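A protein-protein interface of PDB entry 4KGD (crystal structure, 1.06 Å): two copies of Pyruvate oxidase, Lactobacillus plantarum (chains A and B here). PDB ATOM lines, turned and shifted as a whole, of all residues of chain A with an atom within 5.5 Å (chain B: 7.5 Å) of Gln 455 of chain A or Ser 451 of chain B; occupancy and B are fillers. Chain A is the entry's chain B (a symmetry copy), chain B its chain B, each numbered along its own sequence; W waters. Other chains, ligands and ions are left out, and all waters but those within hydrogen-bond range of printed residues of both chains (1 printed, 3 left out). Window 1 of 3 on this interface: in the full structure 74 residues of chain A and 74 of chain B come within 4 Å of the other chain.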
ATOM      1  N   ARG A  57     -13.554  -8.155   8.931  1.00  0.00           N
ATOM      2  CA  ARG A  57     -15.011  -8.190   8.720  1.00  0.00           C
ATOM      3  C   ARG A  57     -15.450  -7.388   7.495  1.00  0.00           C
ATOM      4  O   ARG A  57     -16.623  -7.505   7.123  1.00  0.00           O
ATOM      5  CB  ARG A  57     -15.751  -7.729   9.963  1.00  0.00           C
ATOM      6  CG  ARG A  57     -15.492  -8.518  11.239  1.00  0.00           C
ATOM      7  CD  ARG A  57     -15.461 -10.006  11.129  1.00  0.00           C
ATOM      8  NE  ARG A  57     -15.248 -10.794  12.422  1.00  0.00           N
ATOM      9  CZ  ARG A  57     -16.235 -11.064  13.247  1.00  0.00           C
ATOM     10  NH1 ARG A  57     -17.511 -10.863  12.989  1.00  0.00           N
ATOM     11  NH2 ARG A  57     -15.891 -11.629  14.409  1.00  0.00           N
ATOM     12  N   HIS A  58     -14.555  -6.663   6.858  1.00  0.00           N
ATOM     13  CA  HIS A  58     -14.760  -5.986   5.593  1.00  0.00           C
ATOM     14  C   HIS A  58     -13.390  -5.828   4.955  1.00  0.00           C
ATOM     15  O   HIS A  58     -12.439  -5.411   5.611  1.00  0.00           O
ATOM     16  CB  HIS A  58     -15.445  -4.615   5.842  1.00  0.00           C
ATOM     17  CG  HIS A  58     -15.863  -3.870   4.629  1.00  0.00           C
ATOM     18  ND1 HIS A  58     -15.071  -3.480   3.672  1.00  0.00           N
ATOM     19  CD2 HIS A  58     -17.068  -3.366   4.316  1.00  0.00           C
ATOM     20  CE1 HIS A  58     -15.694  -2.775   2.749  1.00  0.00           C
ATOM     21  NE2 HIS A  58     -16.971  -2.690   3.127  1.00  0.00           N
ATOM     22  N   VAL A  61     -10.906  -2.889   5.388  1.00  0.00           N
ATOM     23  CA  VAL A  61     -10.142  -2.828   6.627  1.00  0.00           C
ATOM     24  C   VAL A  61      -8.840  -3.608   6.456  1.00  0.00           C
ATOM     25  O   VAL A  61      -7.787  -3.178   6.947  1.00  0.00           O
ATOM     26  CB  VAL A  61     -10.989  -3.291   7.811  1.00  0.00           C
ATOM     27  CG1 VAL A  61     -10.150  -3.551   9.079  1.00  0.00           C
ATOM     28  CG2 VAL A  61     -12.090  -2.289   8.072  1.00  0.00           C
ATOM     29  N   SER A 451     -17.864   5.056  12.228  1.00  0.00           N
ATOM     30  CA  SER A 451     -19.009   4.368  11.670  1.00  0.00           C
ATOM     31  C   SER A 451     -18.644   3.545  10.449  1.00  0.00           C
ATOM     32  O   SER A 451     -19.149   2.432  10.289  1.00  0.00           O
ATOM     33  CB  SER A 451     -20.128   5.356  11.300  1.00  0.00           C
ATOM     34  OG  SER A 451     -20.684   5.945  12.441  1.00  0.00           O
ATOM     35  N   MET A 452     -17.823   4.116   9.574  1.00  0.00           N
ATOM     36  CA  MET A 452     -17.532   3.465   8.294  1.00  0.00           C
ATOM     37  C   MET A 452     -16.880   2.111   8.467  1.00  0.00           C
ATOM     38  O   MET A 452     -17.106   1.246   7.615  1.00  0.00           O
ATOM     39  CB  MET A 452     -16.694   4.354   7.401  1.00  0.00           C
ATOM     40  CG  MET A 452     -17.541   5.493   6.829  1.00  0.00           C
ATOM     41  SD  MET A 452     -16.553   6.510   5.738  1.00  0.00           S
ATOM     42  CE  MET A 452     -17.820   7.667   5.181  1.00  0.00           C
ATOM     43  N   THR A 453     -16.068   1.940   9.522  1.00  0.00           N
ATOM     44  CA  THR A 453     -15.365   0.681   9.719  1.00  0.00           C
ATOM     45  C   THR A 453     -15.698   0.022  11.038  1.00  0.00           C
ATOM     46  O   THR A 453     -14.956  -0.852  11.517  1.00  0.00           O
ATOM     47  CB  THR A 453     -13.856   0.854   9.491  1.00  0.00           C
ATOM     48  OG1 THR A 453     -13.368   1.945  10.283  1.00  0.00           O
ATOM     49  CG2 THR A 453     -13.536   1.095   8.035  1.00  0.00           C
ATOM     50  N   MET A 454     -16.856   0.376  11.656  1.00  0.00           N
ATOM     51  CA  MET A 454     -17.185  -0.056  12.989  1.00  0.00           C
ATOM     52  C   MET A 454     -17.193  -1.555  13.176  1.00  0.00           C
ATOM     53  O   MET A 454     -16.889  -2.061  14.251  1.00  0.00           O
ATOM     54  CB  MET A 454     -18.569   0.498  13.426  1.00  0.00           C
ATOM     55  CG  MET A 454     -19.766   0.030  12.584  1.00  0.00           C
ATOM     56  SD  MET A 454     -21.429   0.206  13.294  1.00  0.00           S
ATOM     57  CE  MET A 454     -21.468   1.946  13.586  1.00  0.00           C
ATOM     58  N   GLN A 455     -17.585  -2.307  12.121  1.00  0.00           N
ATOM     59  CA  GLN A 455     -17.680  -3.762  12.275  1.00  0.00           C
ATOM     60  C   GLN A 455     -16.334  -4.388  12.658  1.00  0.00           C
ATOM     61  O   GLN A 455     -16.335  -5.413  13.347  1.00  0.00           O
ATOM     62  CB  GLN A 455     -18.215  -4.404  11.002  1.00  0.00           C
ATOM     63  CG  GLN A 455     -17.286  -4.379   9.845  1.00  0.00           C
ATOM     64  CD  GLN A 455     -16.994  -3.020   9.190  1.00  0.00           C
ATOM     65  OE1 GLN A 455     -17.850  -2.122   9.187  1.00  0.00           O
ATOM     66  NE2 GLN A 455     -15.798  -2.908   8.656  1.00  0.00           N
ATOM     67  N   ASP A 456     -15.226  -3.760  12.255  1.00  0.00           N
ATOM     68  CA  ASP A 456     -13.905  -4.314  12.578  1.00  0.00           C
ATOM     69  C   ASP A 456     -13.430  -3.987  13.973  1.00  0.00           C
ATOM     70  O   ASP A 456     -12.348  -4.435  14.379  1.00  0.00           O
ATOM     71  CB  ASP A 456     -12.897  -4.020  11.450  1.00  0.00           C
ATOM     72  CG  ASP A 456     -13.046  -5.030  10.345  1.00  0.00           C
ATOM     73  OD1 ASP A 456     -12.437  -6.113  10.481  1.00  0.00           O
ATOM     74  OD2 ASP A 456     -13.760  -4.794   9.350  1.00  0.00           O
ATOM     75  N   LEU A 457     -14.255  -3.320  14.787  1.00  0.00           N
ATOM     76  CA  LEU A 457     -14.056  -3.436  16.228  1.00  0.00           C
ATOM     77  C   LEU A 457     -14.079  -4.890  16.647  1.00  0.00           C
ATOM     78  O   LEU A 457     -13.364  -5.293  17.574  1.00  0.00           O
ATOM     79  CB  LEU A 457     -15.073  -2.600  16.980  1.00  0.00           C
ATOM     80  CG  LEU A 457     -14.952  -1.084  16.836  1.00  0.00           C
ATOM     81  CD1 LEU A 457     -16.225  -0.464  17.423  1.00  0.00           C
ATOM     82  CD2 LEU A 457     -13.730  -0.512  17.483  1.00  0.00           C
ATOM     83  N   ALA A 458     -14.893  -5.713  15.969  1.00  0.00           N
ATOM     84  CA  ALA A 458     -14.938  -7.157  16.304  1.00  0.00           C
ATOM     85  C   ALA A 458     -13.604  -7.807  16.054  1.00  0.00           C
ATOM     86  O   ALA A 458     -13.315  -8.812  16.720  1.00  0.00           O
ATOM     87  CB  ALA A 458     -15.979  -7.824  15.487  1.00  0.00           C
ATOM     88  N   THR A 459     -12.790  -7.317  15.133  1.00  0.00           N
ATOM     89  CA  THR A 459     -11.488  -7.895  14.823  1.00  0.00           C
ATOM     90  C   THR A 459     -10.544  -7.641  15.970  1.00  0.00           C
ATOM     91  O   THR A 459      -9.734  -8.522  16.308  1.00  0.00           O
ATOM     92  CB  THR A 459     -10.978  -7.330  13.495  1.00  0.00           C
ATOM     93  OG1 THR A 459     -12.017  -7.610  12.535  1.00  0.00           O
ATOM     94  CG2 THR A 459      -9.651  -7.907  13.047  1.00  0.00           C
ATOM     95  N   VAL A 509     -20.120  -6.057  19.860  1.00  0.00           N
ATOM     96  CA  VAL A 509     -18.978  -6.875  19.416  1.00  0.00           C
ATOM     97  C   VAL A 509     -18.195  -7.468  20.588  1.00  0.00           C
ATOM     98  O   VAL A 509     -17.152  -8.097  20.389  1.00  0.00           O
ATOM     99  CB  VAL A 509     -18.034  -6.100  18.450  1.00  0.00           C
ATOM    100  CG1 VAL A 509     -18.796  -5.528  17.270  1.00  0.00           C
ATOM    101  CG2 VAL A 509     -17.276  -5.007  19.180  1.00  0.00           C
ATOM    102  N   HIS B  58     -22.048   5.180   4.756  1.00  0.00           N
ATOM    103  CA  HIS B  58     -20.933   4.712   3.956  1.00  0.00           C
ATOM    104  C   HIS B  58     -21.383   4.765   2.506  1.00  0.00           C
ATOM    105  O   HIS B  58     -22.477   4.316   2.173  1.00  0.00           O
ATOM    106  CB  HIS B  58     -20.549   3.272   4.391  1.00  0.00           C
ATOM    107  CG  HIS B  58     -19.324   2.712   3.770  1.00  0.00           C
ATOM    108  ND1 HIS B  58     -19.131   2.548   2.493  1.00  0.00           N
ATOM    109  CD2 HIS B  58     -18.241   2.181   4.361  1.00  0.00           C
ATOM    110  CE1 HIS B  58     -17.981   1.965   2.221  1.00  0.00           C
ATOM    111  NE2 HIS B  58     -17.386   1.723   3.390  1.00  0.00           N
ATOM    112  N   GLU B  60     -20.748   3.132  -0.170  1.00  0.00           N
ATOM    113  CA  GLU B  60     -21.116   1.886  -0.824  1.00  0.00           C
ATOM    114  C   GLU B  60     -22.588   1.611  -0.645  1.00  0.00           C
ATOM    115  O   GLU B  60     -23.200   1.061  -1.560  1.00  0.00           O
ATOM    116  CB  GLU B  60     -20.309   0.689  -0.376  1.00  0.00           C
ATOM    117  CG  GLU B  60     -20.755  -0.047   0.858  1.00  0.00           C
ATOM    118  CD  GLU B  60     -19.813  -1.234   1.125  1.00  0.00           C
ATOM    119  OE1 GLU B  60     -19.867  -2.173   0.254  1.00  0.00           O
ATOM    120  OE2 GLU B  60     -19.081  -1.196   2.117  1.00  0.00           O
ATOM    121  N   ASP B 393     -29.360 -10.528   1.161  1.00  0.00           N
ATOM    122  CA  ASP B 393     -27.907 -10.428   1.101  1.00  0.00           C
ATOM    123  C   ASP B 393     -27.346 -11.650   0.382  1.00  0.00           C
ATOM    124  O   ASP B 393     -28.066 -12.301  -0.371  1.00  0.00           O
ATOM    125  CB  ASP B 393     -27.354 -10.191   2.519  1.00  0.00           C
ATOM    126  CG  ASP B 393     -26.104  -9.285   2.552  1.00  0.00           C
ATOM    127  OD1 ASP B 393     -25.018  -9.737   2.109  1.00  0.00           O
ATOM    128  OD2 ASP B 393     -26.241  -8.098   2.954  1.00  0.00           O
ATOM    129  N   MET B 422     -21.703  -9.092  -1.075  1.00  0.00           N
ATOM    130  CA  MET B 422     -22.245  -9.044   0.255  1.00  0.00           C
ATOM    131  C   MET B 422     -22.519  -7.589   0.676  1.00  0.00           C
ATOM    132  O   MET B 422     -21.866  -6.660   0.185  1.00  0.00           O
ATOM    133  CB  MET B 422     -21.298  -9.650   1.269  1.00  0.00           C
ATOM    134  CG  MET B 422     -21.132 -11.186   1.102  1.00  0.00           C
ATOM    135  SD  MET B 422     -19.690 -11.786   2.018  1.00  0.00           S
ATOM    136  CE  MET B 422     -20.136 -11.411   3.695  1.00  0.00           C
ATOM    137  N   GLY B 423     -23.421  -7.441   1.622  1.00  0.00           N
ATOM    138  CA  GLY B 423     -23.761  -6.196   2.247  1.00  0.00           C
ATOM    139  C   GLY B 423     -24.984  -5.535   1.624  1.00  0.00           C
ATOM    140  O   GLY B 423     -25.449  -4.508   2.153  1.00  0.00           O
ATOM    141  N   ILE B 426     -29.084  -4.490   3.592  1.00  0.00           N
ATOM    142  CA  ILE B 426     -29.472  -3.203   4.201  1.00  0.00           C
ATOM    143  C   ILE B 426     -29.810  -2.162   3.130  1.00  0.00           C
ATOM    144  O   ILE B 426     -30.914  -1.593   3.202  1.00  0.00           O
ATOM    145  CB  ILE B 426     -28.425  -2.779   5.226  1.00  0.00           C
ATOM    146  CG1 ILE B 426     -28.496  -3.667   6.477  1.00  0.00           C
ATOM    147  CG2 ILE B 426     -28.534  -1.310   5.569  1.00  0.00           C
ATOM    148  CD1 ILE B 426     -27.310  -3.551   7.413  1.00  0.00           C
ATOM    149  N   ALA B 445     -30.443 -11.253   5.855  1.00  0.00           N
ATOM    150  CA  ALA B 445     -28.996 -11.163   5.681  1.00  0.00           C
ATOM    151  C   ALA B 445     -28.294 -12.115   6.629  1.00  0.00           C
ATOM    152  O   ALA B 445     -28.703 -12.271   7.792  1.00  0.00           O
ATOM    153  CB  ALA B 445     -28.479  -9.758   5.970  1.00  0.00           C
ATOM    154  N   GLY B 446     -27.219 -12.740   6.153  1.00  0.00           N
ATOM    155  CA  GLY B 446     -26.304 -13.437   7.070  1.00  0.00           C
ATOM    156  C   GLY B 446     -25.535 -12.433   7.897  1.00  0.00           C
ATOM    157  O   GLY B 446     -25.478 -11.244   7.631  1.00  0.00           O
ATOM    158  N   ASP B 447     -24.931 -12.954   8.973  1.00  0.00           N
ATOM    159  CA  ASP B 447     -24.135 -12.135   9.869  1.00  0.00           C
ATOM    160  C   ASP B 447     -22.931 -11.510   9.180  1.00  0.00           C
ATOM    161  O   ASP B 447     -22.573 -10.343   9.475  1.00  0.00           O
ATOM    162  CB  ASP B 447     -23.767 -12.864  11.150  1.00  0.00           C
ATOM    163  CG  ASP B 447     -23.149 -14.222  11.072  1.00  0.00           C
ATOM    164  OD1 ASP B 447     -22.983 -14.766   9.950  1.00  0.00           O
ATOM    165  OD2 ASP B 447     -22.863 -14.775  12.164  1.00  0.00           O
ATOM    166  N   GLY B 448     -22.280 -12.224   8.300  1.00  0.00           N
ATOM    167  CA  GLY B 448     -21.160 -11.672   7.573  1.00  0.00           C
ATOM    168  C   GLY B 448     -21.536 -10.483   6.713  1.00  0.00           C
ATOM    169  O   GLY B 448     -20.865  -9.444   6.723  1.00  0.00           O
ATOM    170  N   GLY B 449     -22.605 -10.628   5.963  1.00  0.00           N
ATOM    171  CA  GLY B 449     -23.050  -9.548   5.052  1.00  0.00           C
ATOM    172  C   GLY B 449     -23.673  -8.395   5.803  1.00  0.00           C
ATOM    173  O   GLY B 449     -23.385  -7.237   5.486  1.00  0.00           O
ATOM    174  N   ALA B 450     -24.470  -8.694   6.841  1.00  0.00           N
ATOM    175  CA  ALA B 450     -25.016  -7.611   7.650  1.00  0.00           C
ATOM    176  C   ALA B 450     -23.899  -6.807   8.286  1.00  0.00           C
ATOM    177  O   ALA B 450     -24.012  -5.596   8.435  1.00  0.00           O
ATOM    178  CB  ALA B 450     -25.956  -8.145   8.701  1.00  0.00           C
ATOM    179  N   SER B 451     -22.866  -7.487   8.754  1.00  0.00           N
ATOM    180  CA  SER B 451     -21.733  -6.802   9.339  1.00  0.00           C
ATOM    181  C   SER B 451     -21.148  -5.761   8.404  1.00  0.00           C
ATOM    182  O   SER B 451     -20.771  -4.677   8.854  1.00  0.00           O
ATOM    183  CB  SER B 451     -20.631  -7.795   9.747  1.00  0.00           C
ATOM    184  OG  SER B 451     -21.046  -8.606  10.809  1.00  0.00           O
ATOM    185  N   MET B 452     -21.022  -6.114   7.129  1.00  0.00           N
ATOM    186  CA  MET B 452     -20.331  -5.238   6.180  1.00  0.00           C
ATOM    187  C   MET B 452     -20.999  -3.888   6.045  1.00  0.00           C
ATOM    188  O   MET B 452     -20.288  -2.910   5.792  1.00  0.00           O
ATOM    189  CB  MET B 452     -20.180  -5.900   4.827  1.00  0.00           C
ATOM    190  CG  MET B 452     -19.103  -6.985   4.878  1.00  0.00           C
ATOM    191  SD  MET B 452     -18.899  -7.729   3.263  1.00  0.00           S
ATOM    192  CE  MET B 452     -17.547  -8.867   3.627  1.00  0.00           C
ATOM    193  N   THR B 453     -22.335  -3.836   6.176  1.00  0.00           N
ATOM    194  CA  THR B 453     -23.048  -2.580   6.004  1.00  0.00           C
ATOM    195  C   THR B 453     -23.836  -2.178   7.230  1.00  0.00           C
ATOM    196  O   THR B 453     -24.754  -1.345   7.150  1.00  0.00           O
ATOM    197  CB  THR B 453     -23.891  -2.601   4.720  1.00  0.00           C
ATOM    198  OG1 THR B 453     -24.720  -3.770   4.703  1.00  0.00           O
ATOM    199  CG2 THR B 453     -23.025  -2.569   3.483  1.00  0.00           C
ATOM    200  N   MET B 454     -23.478  -2.716   8.425  1.00  0.00           N
ATOM    201  CA  MET B 454     -24.262  -2.541   9.620  1.00  0.00           C
ATOM    202  C   MET B 454     -24.505  -1.099  10.001  1.00  0.00           C
ATOM    203  O   MET B 454     -25.535  -0.759  10.574  1.00  0.00           O
ATOM    204  CB  MET B 454     -23.603  -3.261  10.827  1.00  0.00           C
ATOM    205  CG  MET B 454     -22.210  -2.748  11.226  1.00  0.00           C
ATOM    206  SD  MET B 454     -21.590  -3.163  12.882  1.00  0.00           S
ATOM    207  CE  MET B 454     -21.648  -4.926  12.811  1.00  0.00           C
ATOM    208  N   GLN B 455     -23.522  -0.211   9.717  1.00  0.00           N
ATOM    209  CA  GLN B 455     -23.678   1.186  10.133  1.00  0.00           C
ATOM    210  C   GLN B 455     -24.918   1.837   9.506  1.00  0.00           C
ATOM    211  O   GLN B 455     -25.497   2.728  10.135  1.00  0.00           O
ATOM    212  CB  GLN B 455     -22.433   1.991   9.791  1.00  0.00           C
ATOM    213  CG  GLN B 455     -22.213   2.231   8.343  1.00  0.00           C
ATOM    214  CD  GLN B 455     -21.831   1.026   7.469  1.00  0.00           C
ATOM    215  OE1 GLN B 455     -21.183   0.080   7.942  1.00  0.00           O
ATOM    216  NE2 GLN B 455     -22.244   1.095   6.222  1.00  0.00           N
ATOM    217  N   VAL B 471     -31.312 -11.050  10.770  1.00  0.00           N
ATOM    218  CA  VAL B 471     -29.919 -11.444  10.638  1.00  0.00           C
ATOM    219  C   VAL B 471     -29.808 -12.878  11.072  1.00  0.00           C
ATOM    220  O   VAL B 471     -30.319 -13.304  12.108  1.00  0.00           O
ATOM    221  CB  VAL B 471     -28.978 -10.548  11.477  1.00  0.00           C
ATOM    222  CG1 VAL B 471     -27.531 -11.005  11.329  1.00  0.00           C
ATOM    223  CG2 VAL B 471     -29.135  -9.091  11.081  1.00  0.00           C
ATOM    224  N   TYR B 477     -18.886 -17.592   7.920  1.00  0.00           N
ATOM    225  CA  TYR B 477     -19.174 -17.414   6.488  1.00  0.00           C
ATOM    226  C   TYR B 477     -19.608 -18.813   6.003  1.00  0.00           C
ATOM    227  O   TYR B 477     -18.799 -19.561   5.437  1.00  0.00           O
ATOM    228  CB  TYR B 477     -17.946 -16.926   5.727  1.00  0.00           C
ATOM    229  CG  TYR B 477     -17.461 -15.549   6.138  1.00  0.00           C
ATOM    230  CD1 TYR B 477     -18.300 -14.431   6.157  1.00  0.00           C
ATOM    231  CD2 TYR B 477     -16.155 -15.331   6.478  1.00  0.00           C
ATOM    232  CE1 TYR B 477     -17.846 -13.182   6.512  1.00  0.00           C
ATOM    233  CE2 TYR B 477     -15.705 -14.095   6.857  1.00  0.00           C
ATOM    234  CZ  TYR B 477     -16.541 -13.001   6.873  1.00  0.00           C
ATOM    235  OH  TYR B 477     -16.049 -11.794   7.264  1.00  0.00           O
ATOM    236  N   PHE B 497     -15.965 -17.398  13.118  1.00  0.00           N
ATOM    237  CA  PHE B 497     -15.515 -16.162  13.756  1.00  0.00           C
ATOM    238  C   PHE B 497     -16.372 -15.887  14.985  1.00  0.00           C
ATOM    239  O   PHE B 497     -17.280 -16.598  15.342  1.00  0.00           O
ATOM    240  CB  PHE B 497     -15.473 -15.026  12.736  1.00  0.00           C
ATOM    241  CG  PHE B 497     -16.740 -14.857  11.927  1.00  0.00           C
ATOM    242  CD1 PHE B 497     -17.950 -14.472  12.486  1.00  0.00           C
ATOM    243  CD2 PHE B 497     -16.720 -15.069  10.567  1.00  0.00           C
ATOM    244  CE1 PHE B 497     -19.069 -14.307  11.722  1.00  0.00           C
ATOM    245  CE2 PHE B 497     -17.847 -14.892   9.787  1.00  0.00           C
ATOM    246  CZ  PHE B 497     -19.029 -14.492  10.362  1.00  0.00           C
ATOM    247  N   ASN B 498     -15.997 -14.825  15.722  1.00  0.00           N
ATOM    248  CA  ASN B 498     -16.604 -14.457  16.975  1.00  0.00           C
ATOM    249  C   ASN B 498     -17.953 -13.747  16.744  1.00  0.00           C
ATOM    250  O   ASN B 498     -18.084 -12.928  15.838  1.00  0.00           O
ATOM    251  CB  ASN B 498     -15.722 -13.492  17.776  1.00  0.00           C
ATOM    252  CG  ASN B 498     -14.471 -14.125  18.284  1.00  0.00           C
ATOM    253  OD1 ASN B 498     -14.136 -15.258  18.024  1.00  0.00           O
ATOM    254  ND2 ASN B 498     -13.762 -13.369  19.116  1.00  0.00           N
ATOM    255  N   ILE B 500     -21.226 -11.423  16.889  1.00  0.00           N
ATOM    256  CA  ILE B 500     -21.694 -10.061  17.060  1.00  0.00           C
ATOM    257  C   ILE B 500     -23.177 -10.132  17.405  1.00  0.00           C
ATOM    258  O   ILE B 500     -23.946 -10.833  16.740  1.00  0.00           O
ATOM    259  CB  ILE B 500     -21.489  -9.212  15.807  1.00  0.00           C
ATOM    260  CG1 ILE B 500     -20.020  -9.061  15.477  1.00  0.00           C
ATOM    261  CG2 ILE B 500     -22.214  -7.857  15.935  1.00  0.00           C
ATOM    262  CD1 ILE B 500     -19.695  -8.260  14.232  1.00  0.00           C
ATOM    263  N   PHE B 502     -26.317  -8.514  17.115  1.00  0.00           N
ATOM    264  CA  PHE B 502     -26.922  -7.493  16.283  1.00  0.00           C
ATOM    265  C   PHE B 502     -28.106  -6.822  16.989  1.00  0.00           C
ATOM    266  O   PHE B 502     -28.499  -5.725  16.582  1.00  0.00           O
ATOM    267  CB  PHE B 502     -27.370  -8.005  14.911  1.00  0.00           C
ATOM    268  CG  PHE B 502     -26.303  -7.915  13.902  1.00  0.00           C
ATOM    269  CD1 PHE B 502     -26.209  -6.766  13.153  1.00  0.00           C
ATOM    270  CD2 PHE B 502     -25.439  -8.989  13.765  1.00  0.00           C
ATOM    271  CE1 PHE B 502     -25.200  -6.659  12.189  1.00  0.00           C
ATOM    272  CE2 PHE B 502     -24.416  -8.896  12.833  1.00  0.00           C
ATOM    273  CZ  PHE B 502     -24.325  -7.722  12.086  1.00  0.00           C
ATOM    274  N   ILE B 505     -26.126  -4.027  18.412  1.00  0.00           N
ATOM    275  CA  ILE B 505     -25.829  -3.099  17.334  1.00  0.00           C
ATOM    276  C   ILE B 505     -27.044  -2.232  17.018  1.00  0.00           C
ATOM    277  O   ILE B 505     -26.967  -0.993  16.910  1.00  0.00           O
ATOM    278  CB  ILE B 505     -25.349  -3.853  16.083  1.00  0.00           C
ATOM    279  CG1 ILE B 505     -24.118  -4.698  16.296  1.00  0.00           C
ATOM    280  CG2 ILE B 505     -25.172  -2.865  14.919  1.00  0.00           C
ATOM    281  CD1 ILE B 505     -22.894  -3.954  16.733  1.00  0.00           C
HETATM  282  O   HOH W   1     -18.031  -9.834   7.437  1.00  0.00           O
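Of the 24 printed residues of chain B, 9 touch a printed residue of chain A.
Hydrophobic or aromatic side chains of chain B within 4 Å of the printed part of chain A: His 58, Met 452, Met 454, Phe 497 and Ile 500.
Hydrophobic or aromatic side chains of chain A that line the printed part of chain B: His 58, Met 454 and Ala 458.
Water W1 lies within hydrogen-bond range of O of Arg 57 of chain A, OH of Tyr 477 of chain B and O of Gly 448 of chain B.
Of the printed residues of chain B, Met 454 of chain A touches Met 454 and Gln 455.
Of the printed residues of chain B, Gln 455 of chain A touches Ser 451 (3.3 Å) and Met 454 (3.9 Å).
Printed residues of chain B within 4 Å of Ala 458 of chain A: Ile 500 (3.9 Å).
Printed residues of chain A within 4 Å of Ser 451 of chain B: Gln 455 (3.3 Å).
Printed residues of chain A within 4 Å of Met 452 of chain B: Arg 57 (3.4 Å) and His 58 (3.6 Å).
The nearest printed residue of chain B that does not touch Gln 455 of chain A is Gln 455 of chain B (4.2 Å).
The nearest printed residue of chain A that does not touch Ser 451 of chain B is Arg 57 of chain A (4.7 Å).
The nearest printed residue of chain B that does not touch Arg 57 of chain A is Tyr 477 of chain B (4.02 Å).
N of Arg 57 of chain A sits at hydrogen-bond distance from OD1 of Asp 456 of chain A.
A ring nitrogen (ND1) of His 58 of chain B sits at hydrogen-bond distance from the backbone NH (N) of Glu 60 of chain B (3.2 Å).
The side-chain carboxylate (OD2) of Asp 456 of chain A is in hydrogen-bond range of the backbone NH (N) of His 58 of chain A (3.2 Å).
The side-chain amide nitrogen of Gln 455 of chain A is in hydrogen-bond range of the side-chain carboxylate of Asp 456 of chain A, at 2.9 Å.
The backbone carbonyl oxygen (O) of Asp 447 of chain B lies within hydrogen-bond range of the side-chain hydroxyl (OG) of Ser 451 of chain B, at 2.7 Å.
O of Asn 498 of chain B lies within hydrogen-bond range of NH2 of Arg 57 of chain A (2.9 Å).
The side-chain carboxylate (OE2) of Glu 60 of chain B is in hydrogen-bond range of a ring nitrogen (NE2) of His 58 of chain A (2.8 Å).
The side-chain sulfur (SD) of Met 454 of chain B sits close to the side-chain sulfur (SD) of Met 454 of chain A.
Among the printed residues, pairs that only touch across the chains: Arg 57 of chain A with Met 452 of chain B (3.4 Å), Arg 57 of chain A with Phe 497 of chain B (3.7 Å), Arg 57 of chain A with Ile 500 of chain B (3.6 Å), His 58 of chain A with Met 452 of chain B (3.6 Å), Ser 451 of chain A with Gln 455 of chain B (3.4 Å), Met 452 of chain A with His 58 of chain B (3.6 Å), Met 454 of chain A with Gln 455 of chain B (3.9 Å), Gln 455 of chain A with Ser 451 of chain B (3.3 Å), Gln 455 of chain A with Met 454 of chain B (3.9 Å) and Ala 458 of chain A with Ile 500 of chain B (3.9 Å).
His 58 of chain A touches Met 452 of chain B, and with the chains exchanged Met 452 of chain A touches His 58 of chain B.
Ser 451 of chain A touches Gln 455 of chain B, and with the chains exchanged Gln 455 of chain A touches Ser 451 of chain B.
Met 454 of chain A touches its own counterpart, Met 454 of chain B.
Met 454 of chain A touches Gln 455 of chain B, and with the chains exchanged Gln 455 of chain A touches Met 454 of chain B.
6 positions are printed for both chains.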
